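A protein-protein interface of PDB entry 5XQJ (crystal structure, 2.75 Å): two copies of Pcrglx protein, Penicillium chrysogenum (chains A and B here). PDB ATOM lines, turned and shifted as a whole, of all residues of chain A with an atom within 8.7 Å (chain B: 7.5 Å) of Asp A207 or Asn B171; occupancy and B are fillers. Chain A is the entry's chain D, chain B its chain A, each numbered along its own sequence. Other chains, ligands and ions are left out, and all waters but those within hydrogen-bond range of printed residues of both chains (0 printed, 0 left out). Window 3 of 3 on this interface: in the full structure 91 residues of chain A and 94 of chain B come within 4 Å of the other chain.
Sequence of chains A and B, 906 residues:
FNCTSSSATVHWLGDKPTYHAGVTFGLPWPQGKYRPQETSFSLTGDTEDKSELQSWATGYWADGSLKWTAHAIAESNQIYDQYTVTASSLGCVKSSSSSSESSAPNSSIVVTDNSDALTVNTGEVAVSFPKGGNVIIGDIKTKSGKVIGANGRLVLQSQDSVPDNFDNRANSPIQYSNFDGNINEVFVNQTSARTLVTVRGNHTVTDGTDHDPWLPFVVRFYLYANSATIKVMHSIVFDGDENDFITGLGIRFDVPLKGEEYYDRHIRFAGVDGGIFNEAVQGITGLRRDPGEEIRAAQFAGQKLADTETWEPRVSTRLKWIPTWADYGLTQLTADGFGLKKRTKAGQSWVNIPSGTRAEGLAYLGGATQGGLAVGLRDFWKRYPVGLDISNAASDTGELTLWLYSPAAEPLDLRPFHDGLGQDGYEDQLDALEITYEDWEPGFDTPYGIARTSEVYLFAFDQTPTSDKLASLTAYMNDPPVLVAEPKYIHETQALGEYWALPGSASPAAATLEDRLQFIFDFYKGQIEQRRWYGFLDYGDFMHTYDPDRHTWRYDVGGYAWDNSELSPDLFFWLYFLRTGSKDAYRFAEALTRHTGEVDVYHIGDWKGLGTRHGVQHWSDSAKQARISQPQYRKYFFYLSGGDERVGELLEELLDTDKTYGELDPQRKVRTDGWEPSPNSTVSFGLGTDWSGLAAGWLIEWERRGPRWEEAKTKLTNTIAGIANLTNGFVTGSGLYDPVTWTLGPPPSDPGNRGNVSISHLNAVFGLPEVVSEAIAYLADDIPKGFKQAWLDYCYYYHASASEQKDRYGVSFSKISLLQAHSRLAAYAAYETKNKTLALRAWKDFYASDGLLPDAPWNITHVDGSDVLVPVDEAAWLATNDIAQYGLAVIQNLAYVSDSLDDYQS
The side-chain amide nitrogen of Asn A178 sits at hydrogen-bond distance from the backbone carbonyl oxygen of Asp B167 (3.0 Å). The guanidinium group of Arg B169 lies close to the side-chain amide oxygen of Gln A157 (3.2 Å). The side-chain amide nitrogen (ND2) of Asn B171 sits at hydrogen-bond distance from the side-chain carboxylate (OD2) of Asp A207, 2.8 Å away.
The backbone NH (N) of Asn A178 lies within hydrogen-bond range of the backbone carbonyl oxygen (O) of Asp A207 (3.3 Å). The backbone carbonyl oxygen (O) of Tyr A176 sits at hydrogen-bond distance from the backbone NH (N) of Thr A209, 3.1 Å away. The side-chain amide oxygen (OD1) of Asn A178 sits at hydrogen-bond distance from the side-chain amide nitrogen (NE2) of Gln A157, 3.2 Å away. The backbone NH of Thr A206 lies within hydrogen-bond range of the backbone carbonyl oxygen of Asn A178, at 3.0 Å.
Among the printed residues, merely in contact across the chains: Gln A157 with Phe B166, Gly A208 with Ala B170, Asn A178 with Ala B170, Tyr A176 with Arg B169 and Tyr A176 with Ala B170.
Asp A207 touches just one residue of chain B: Asn B171. Of chain A, only Asp A207 (2.8 Å) comes within 4 Å of Asn B171. Printed residues of chain A within 4 Å of Arg B169: Gln A157 (3.1 Å) and Tyr A176 (3.8 Å). Printed residues of chain B within 4 Å of Asn A178: Asp B167 and Ala B170. The nearest residue of chain B that does not touch Asp A207 is Ala B170 (4.1 Å).
Hydrophobic or aromatic side chains of chain B within 4 Å of the printed part of chain A: Ala B170. Along chain B the printed residues that touch a printed residue of chain A span positions 166 to 171. Among the printed residues, 8 pairs touch across the chains. Among the printed residues, no Asp or Glu carboxylate lies within 4 Å of a Lys or Arg side-chain nitrogen of the other chain.
No position is printed for both chains.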
ATOM      1  N   LEU A 156      18.854  -6.658 -10.811  1.00  0.00           N
ATOM      2  CA  LEU A 156      19.215  -5.919  -9.627  1.00  0.00           C
ATOM      3  C   LEU A 156      19.146  -6.948  -8.514  1.00  0.00           C
ATOM      4  O   LEU A 156      18.220  -7.763  -8.501  1.00  0.00           O
ATOM      5  CB  LEU A 156      18.210  -4.804  -9.357  1.00  0.00           C
ATOM      6  CG  LEU A 156      18.235  -4.114  -7.963  1.00  0.00           C
ATOM      7  CD1 LEU A 156      19.501  -3.307  -7.697  1.00  0.00           C
ATOM      8  CD2 LEU A 156      17.033  -3.206  -7.715  1.00  0.00           C
ATOM      9  N   GLN A 157      20.122  -6.968  -7.609  1.00  0.00           N
ATOM     10  CA  GLN A 157      19.928  -7.747  -6.384  1.00  0.00           C
ATOM     11  C   GLN A 157      20.461  -6.977  -5.225  1.00  0.00           C
ATOM     12  O   GLN A 157      21.265  -6.079  -5.372  1.00  0.00           O
ATOM     13  CB  GLN A 157      20.373  -9.247  -6.426  1.00  0.00           C
ATOM     14  CG  GLN A 157      21.854  -9.618  -6.403  1.00  0.00           C
ATOM     15  CD  GLN A 157      22.183 -10.767  -5.418  1.00  0.00           C
ATOM     16  OE1 GLN A 157      23.338 -11.180  -5.251  1.00  0.00           O
ATOM     17  NE2 GLN A 157      21.170 -11.256  -4.754  1.00  0.00           N
ATOM     18  N   SER A 158      19.871  -7.253  -4.070  1.00  0.00           N
ATOM     19  CA  SER A 158      20.101  -6.446  -2.872  1.00  0.00           C
ATOM     20  C   SER A 158      20.082  -7.326  -1.623  1.00  0.00           C
ATOM     21  O   SER A 158      19.679  -8.494  -1.679  1.00  0.00           O
ATOM     22  CB  SER A 158      19.038  -5.334  -2.786  1.00  0.00           C
ATOM     23  OG  SER A 158      17.769  -5.829  -2.399  1.00  0.00           O
ATOM     24  N   GLN A 175      19.751 -11.566   4.036  1.00  0.00           N
ATOM     25  CA  GLN A 175      18.617 -11.984   3.243  1.00  0.00           C
ATOM     26  C   GLN A 175      18.689 -11.305   1.862  1.00  0.00           C
ATOM     27  O   GLN A 175      18.556 -10.075   1.733  1.00  0.00           O
ATOM     28  CB  GLN A 175      17.301 -11.720   3.994  1.00  0.00           C
ATOM     29  CG  GLN A 175      17.056 -12.674   5.179  1.00  0.00           C
ATOM     30  CD  GLN A 175      15.594 -12.669   5.668  1.00  0.00           C
ATOM     31  OE1 GLN A 175      15.209 -11.841   6.507  1.00  0.00           O
ATOM     32  NE2 GLN A 175      14.767 -13.594   5.130  1.00  0.00           N
ATOM     33  N   TYR A 176      18.910 -12.140   0.844  1.00  0.00           N
ATOM     34  CA  TYR A 176      19.019 -11.691  -0.537  1.00  0.00           C
ATOM     35  C   TYR A 176      17.693 -11.568  -1.263  1.00  0.00           C
ATOM     36  O   TYR A 176      16.788 -12.382  -1.078  1.00  0.00           O
ATOM     37  CB  TYR A 176      19.896 -12.648  -1.333  1.00  0.00           C
ATOM     38  CG  TYR A 176      21.331 -12.557  -0.945  1.00  0.00           C
ATOM     39  CD1 TYR A 176      22.123 -11.546  -1.452  1.00  0.00           C
ATOM     40  CD2 TYR A 176      21.897 -13.465  -0.037  1.00  0.00           C
ATOM     41  CE1 TYR A 176      23.457 -11.431  -1.092  1.00  0.00           C
ATOM     42  CE2 TYR A 176      23.237 -13.383   0.317  1.00  0.00           C
ATOM     43  CZ  TYR A 176      24.018 -12.354  -0.218  1.00  0.00           C
ATOM     44  OH  TYR A 176      25.344 -12.208   0.129  1.00  0.00           O
ATOM     45  N   SER A 177      17.622 -10.570  -2.140  1.00  0.00           N
ATOM     46  CA  SER A 177      16.462 -10.328  -2.958  1.00  0.00           C
ATOM     47  C   SER A 177      16.890 -10.009  -4.383  1.00  0.00           C
ATOM     48  O   SER A 177      17.683  -9.116  -4.572  1.00  0.00           O
ATOM     49  CB  SER A 177      15.706  -9.141  -2.375  1.00  0.00           C
ATOM     50  OG  SER A 177      15.619  -9.261  -0.977  1.00  0.00           O
ATOM     51  N   ASN A 178      16.378 -10.744  -5.369  1.00  0.00           N
ATOM     52  CA  ASN A 178      16.524 -10.384  -6.805  1.00  0.00           C
ATOM     53  C   ASN A 178      15.297  -9.635  -7.318  1.00  0.00           C
ATOM     54  O   ASN A 178      14.172  -9.833  -6.846  1.00  0.00           O
ATOM     55  CB  ASN A 178      16.712 -11.611  -7.726  1.00  0.00           C
ATOM     56  CG  ASN A 178      17.824 -12.522  -7.273  1.00  0.00           C
ATOM     57  OD1 ASN A 178      18.846 -12.078  -6.734  1.00  0.00           O
ATOM     58  ND2 ASN A 178      17.640 -13.818  -7.501  1.00  0.00           N
ATOM     59  N   PHE A 179      15.550  -8.822  -8.338  1.00  0.00           N
ATOM     60  CA  PHE A 179      14.575  -7.959  -8.918  1.00  0.00           C
ATOM     61  C   PHE A 179      14.755  -7.882 -10.450  1.00  0.00           C
ATOM     62  O   PHE A 179      15.761  -8.320 -11.007  1.00  0.00           O
ATOM     63  CB  PHE A 179      14.769  -6.558  -8.374  1.00  0.00           C
ATOM     64  CG  PHE A 179      14.557  -6.394  -6.902  1.00  0.00           C
ATOM     65  CD1 PHE A 179      15.534  -6.764  -6.011  1.00  0.00           C
ATOM     66  CD2 PHE A 179      13.432  -5.716  -6.410  1.00  0.00           C
ATOM     67  CE1 PHE A 179      15.388  -6.542  -4.651  1.00  0.00           C
ATOM     68  CE2 PHE A 179      13.272  -5.468  -5.052  1.00  0.00           C
ATOM     69  CZ  PHE A 179      14.263  -5.888  -4.169  1.00  0.00           C
ATOM     70  N   ASP A 180      13.765  -7.256 -11.082  1.00  0.00           N
ATOM     71  CA  ASP A 180      13.547  -7.189 -12.518  1.00  0.00           C
ATOM     72  C   ASP A 180      13.088  -5.796 -12.886  1.00  0.00           C
ATOM     73  O   ASP A 180      12.430  -5.142 -12.103  1.00  0.00           O
ATOM     74  CB  ASP A 180      12.358  -8.098 -12.859  1.00  0.00           C
ATOM     75  CG  ASP A 180      12.736  -9.227 -13.704  1.00  0.00           C
ATOM     76  OD1 ASP A 180      13.948  -9.343 -13.969  1.00  0.00           O
ATOM     77  OD2 ASP A 180      11.832  -9.992 -14.111  1.00  0.00           O
ATOM     78  N   THR A 204      10.948  -4.485  -9.627  1.00  0.00           N
ATOM     79  CA  THR A 204      10.082  -5.370  -8.823  1.00  0.00           C
ATOM     80  C   THR A 204      10.716  -6.758  -8.449  1.00  0.00           C
ATOM     81  O   THR A 204      11.380  -7.389  -9.279  1.00  0.00           O
ATOM     82  CB  THR A 204       8.769  -5.659  -9.578  1.00  0.00           C
ATOM     83  OG1 THR A 204       9.022  -6.553 -10.665  1.00  0.00           O
ATOM     84  CG2 THR A 204       8.139  -4.398 -10.116  1.00  0.00           C
ATOM     85  N   VAL A 205      10.492  -7.231  -7.215  1.00  0.00           N
ATOM     86  CA  VAL A 205      10.912  -8.595  -6.813  1.00  0.00           C
ATOM     87  C   VAL A 205      10.620  -9.711  -7.779  1.00  0.00           C
ATOM     88  O   VAL A 205       9.663  -9.673  -8.532  1.00  0.00           O
ATOM     89  CB  VAL A 205      10.295  -9.156  -5.500  1.00  0.00           C
ATOM     90  CG1 VAL A 205      11.377  -9.264  -4.440  1.00  0.00           C
ATOM     91  CG2 VAL A 205       9.069  -8.395  -5.029  1.00  0.00           C
ATOM     92  N   THR A 206      11.466 -10.725  -7.684  1.00  0.00           N
ATOM     93  CA  THR A 206      11.265 -12.016  -8.331  1.00  0.00           C
ATOM     94  C   THR A 206      11.503 -13.028  -7.209  1.00  0.00           C
ATOM     95  O   THR A 206      10.638 -13.237  -6.391  1.00  0.00           O
ATOM     96  CB  THR A 206      12.210 -12.178  -9.562  1.00  0.00           C
ATOM     97  OG1 THR A 206      13.567 -11.834  -9.204  1.00  0.00           O
ATOM     98  CG2 THR A 206      11.743 -11.269 -10.699  1.00  0.00           C
ATOM     99  N   ASP A 207      12.701 -13.565  -7.102  1.00  0.00           N
ATOM    100  CA  ASP A 207      13.042 -14.490  -6.023  1.00  0.00           C
ATOM    101  C   ASP A 207      13.505 -13.740  -4.756  1.00  0.00           C
ATOM    102  O   ASP A 207      13.701 -12.530  -4.758  1.00  0.00           O
ATOM    103  CB  ASP A 207      14.165 -15.450  -6.495  1.00  0.00           C
ATOM    104  CG  ASP A 207      13.820 -16.168  -7.789  1.00  0.00           C
ATOM    105  OD1 ASP A 207      13.888 -15.540  -8.865  1.00  0.00           O
ATOM    106  OD2 ASP A 207      13.474 -17.361  -7.731  1.00  0.00           O
ATOM    107  N   GLY A 208      13.713 -14.496  -3.691  1.00  0.00           N
ATOM    108  CA  GLY A 208      14.293 -13.966  -2.486  1.00  0.00           C
ATOM    109  C   GLY A 208      13.259 -13.348  -1.571  1.00  0.00           C
ATOM    110  O   GLY A 208      12.060 -13.481  -1.778  1.00  0.00           O
ATOM    111  N   THR A 209      13.764 -12.678  -0.541  1.00  0.00           N
ATOM    112  CA  THR A 209      12.956 -12.069   0.498  1.00  0.00           C
ATOM    113  C   THR A 209      12.163 -10.898  -0.138  1.00  0.00           C
ATOM    114  O   THR A 209      12.639 -10.244  -1.074  1.00  0.00           O
ATOM    115  CB  THR A 209      13.847 -11.703   1.733  1.00  0.00           C
ATOM    116  OG1 THR A 209      13.056 -11.320   2.847  1.00  0.00           O
ATOM    117  CG2 THR A 209      14.774 -10.552   1.463  1.00  0.00           C
ATOM    118  N   ASP A 210      10.942 -10.682   0.350  1.00  0.00           N
ATOM    119  CA  ASP A 210       9.982  -9.760  -0.256  1.00  0.00           C
ATOM    120  C   ASP A 210      10.356  -8.276  -0.046  1.00  0.00           C
ATOM    121  O   ASP A 210      10.887  -7.923   0.997  1.00  0.00           O
ATOM    122  CB  ASP A 210       8.590 -10.043   0.323  1.00  0.00           C
ATOM    123  CG  ASP A 210       7.483  -9.505  -0.547  1.00  0.00           C
ATOM    124  OD1 ASP A 210       7.456  -9.817  -1.765  1.00  0.00           O
ATOM    125  OD2 ASP A 210       6.636  -8.770  -0.005  1.00  0.00           O
ATOM    126  N   HIS A 211      10.061  -7.424  -1.039  1.00  0.00           N
ATOM    127  CA  HIS A 211      10.491  -5.989  -1.060  1.00  0.00           C
ATOM    128  C   HIS A 211       9.544  -5.176  -1.975  1.00  0.00           C
ATOM    129  O   HIS A 211       9.123  -5.649  -3.038  1.00  0.00           O
ATOM    130  CB  HIS A 211      11.949  -5.915  -1.585  1.00  0.00           C
ATOM    131  CG  HIS A 211      12.683  -4.630  -1.294  1.00  0.00           C
ATOM    132  ND1 HIS A 211      12.416  -3.439  -1.945  1.00  0.00           N
ATOM    133  CD2 HIS A 211      13.741  -4.381  -0.487  1.00  0.00           C
ATOM    134  CE1 HIS A 211      13.238  -2.503  -1.502  1.00  0.00           C
ATOM    135  NE2 HIS A 211      14.056  -3.052  -0.621  1.00  0.00           N
ATOM    136  N   PRO B 163      26.395 -21.046  -3.842  1.00  0.00           N
ATOM    137  CA  PRO B 163      25.379 -21.034  -4.914  1.00  0.00           C
ATOM    138  C   PRO B 163      25.932 -21.294  -6.309  1.00  0.00           C
ATOM    139  O   PRO B 163      27.044 -20.908  -6.613  1.00  0.00           O
ATOM    140  CB  PRO B 163      24.797 -19.627  -4.853  1.00  0.00           C
ATOM    141  CG  PRO B 163      25.181 -19.106  -3.492  1.00  0.00           C
ATOM    142  CD  PRO B 163      26.493 -19.747  -3.163  1.00  0.00           C
ATOM    143  N   PHE B 166      25.254 -15.895  -9.010  1.00  0.00           N
ATOM    144  CA  PHE B 166      24.906 -14.745  -8.161  1.00  0.00           C
ATOM    145  C   PHE B 166      23.402 -14.656  -7.894  1.00  0.00           C
ATOM    146  O   PHE B 166      22.971 -14.444  -6.759  1.00  0.00           O
ATOM    147  CB  PHE B 166      25.407 -13.446  -8.804  1.00  0.00           C
ATOM    148  CG  PHE B 166      26.908 -13.378  -8.992  1.00  0.00           C
ATOM    149  CD1 PHE B 166      27.798 -13.808  -7.986  1.00  0.00           C
ATOM    150  CD2 PHE B 166      27.443 -12.856 -10.169  1.00  0.00           C
ATOM    151  CE1 PHE B 166      29.165 -13.715  -8.150  1.00  0.00           C
ATOM    152  CE2 PHE B 166      28.812 -12.747 -10.334  1.00  0.00           C
ATOM    153  CZ  PHE B 166      29.664 -13.163  -9.315  1.00  0.00           C
ATOM    154  N   ASP B 167      22.619 -14.816  -8.956  1.00  0.00           N
ATOM    155  CA  ASP B 167      21.160 -15.017  -8.865  1.00  0.00           C
ATOM    156  C   ASP B 167      20.711 -16.078  -7.820  1.00  0.00           C
ATOM    157  O   ASP B 167      19.775 -15.845  -7.049  1.00  0.00           O
ATOM    158  CB  ASP B 167      20.570 -15.331 -10.260  1.00  0.00           C
ATOM    159  CG  ASP B 167      20.637 -14.119 -11.217  1.00  0.00           C
ATOM    160  OD1 ASP B 167      21.675 -13.395 -11.267  1.00  0.00           O
ATOM    161  OD2 ASP B 167      19.633 -13.909 -11.935  1.00  0.00           O
ATOM    162  N   ASN B 168      21.418 -17.193  -7.738  1.00  0.00           N
ATOM    163  CA  ASN B 168      21.009 -18.306  -6.909  1.00  0.00           C
ATOM    164  C   ASN B 168      21.178 -18.029  -5.392  1.00  0.00           C
ATOM    165  O   ASN B 168      20.723 -18.816  -4.570  1.00  0.00           O
ATOM    166  CB  ASN B 168      21.809 -19.551  -7.338  1.00  0.00           C
ATOM    167  CG  ASN B 168      21.278 -20.858  -6.749  1.00  0.00           C
ATOM    168  OD1 ASN B 168      22.059 -21.734  -6.342  1.00  0.00           O
ATOM    169  ND2 ASN B 168      19.960 -21.013  -6.722  1.00  0.00           N
ATOM    170  N   ARG B 169      21.846 -16.941  -5.011  1.00  0.00           N
ATOM    171  CA  ARG B 169      21.947 -16.558  -3.600  1.00  0.00           C
ATOM    172  C   ARG B 169      20.589 -16.508  -2.907  1.00  0.00           C
ATOM    173  O   ARG B 169      20.445 -16.953  -1.789  1.00  0.00           O
ATOM    174  CB  ARG B 169      22.599 -15.169  -3.463  1.00  0.00           C
ATOM    175  CG  ARG B 169      24.095 -15.148  -3.688  1.00  0.00           C
ATOM    176  CD  ARG B 169      24.587 -13.743  -3.974  1.00  0.00           C
ATOM    177  NE  ARG B 169      26.029 -13.702  -4.156  1.00  0.00           N
ATOM    178  CZ  ARG B 169      26.773 -12.607  -4.071  1.00  0.00           C
ATOM    179  NH1 ARG B 169      26.224 -11.415  -3.818  1.00  0.00           N
ATOM    180  NH2 ARG B 169      28.086 -12.705  -4.235  1.00  0.00           N
ATOM    181  N   ALA B 170      19.614 -15.921  -3.584  1.00  0.00           N
ATOM    182  CA  ALA B 170      18.261 -15.756  -3.052  1.00  0.00           C
ATOM    183  C   ALA B 170      17.546 -17.072  -2.744  1.00  0.00           C
ATOM    184  O   ALA B 170      16.599 -17.081  -1.979  1.00  0.00           O
ATOM    185  CB  ALA B 170      17.436 -14.944  -4.030  1.00  0.00           C
ATOM    186  N   ASN B 171      17.985 -18.169  -3.347  1.00  0.00           N
ATOM    187  CA  ASN B 171      17.365 -19.476  -3.150  1.00  0.00           C
ATOM    188  C   ASN B 171      18.314 -20.543  -2.663  1.00  0.00           C
ATOM    189  O   ASN B 171      18.011 -21.729  -2.780  1.00  0.00           O
ATOM    190  CB  ASN B 171      16.736 -19.910  -4.475  1.00  0.00           C
ATOM    191  CG  ASN B 171      15.475 -19.129  -4.785  1.00  0.00           C
ATOM    192  OD1 ASN B 171      14.668 -18.827  -3.862  1.00  0.00           O
ATOM    193  ND2 ASN B 171      15.271 -18.806  -6.078  1.00  0.00           N
ATOM    194  N   SER B 172      19.456 -20.131  -2.107  1.00  0.00           N
ATOM    195  CA  SER B 172      20.553 -21.070  -1.757  1.00  0.00           C
ATOM    196  C   SER B 172      21.323 -20.533  -0.541  1.00  0.00           C
ATOM    197  O   SER B 172      22.295 -19.805  -0.674  1.00  0.00           O
ATOM    198  CB  SER B 172      21.456 -21.304  -2.959  1.00  0.00           C
ATOM    199  OG  SER B 172      22.000 -22.574  -2.876  1.00  0.00           O
ATOM    200  N   PRO B 173      20.838 -20.856   0.656  1.00  0.00           N
ATOM    201  CA  PRO B 173      21.371 -20.115   1.782  1.00  0.00           C
ATOM    202  C   PRO B 173      22.712 -20.676   2.171  1.00  0.00           C
ATOM    203  O   PRO B 173      22.977 -21.872   1.960  1.00  0.00           O
ATOM    204  CB  PRO B 173      20.320 -20.324   2.891  1.00  0.00           C
ATOM    205  CG  PRO B 173      19.402 -21.407   2.394  1.00  0.00           C
ATOM    206  CD  PRO B 173      19.914 -21.925   1.086  1.00  0.00           C
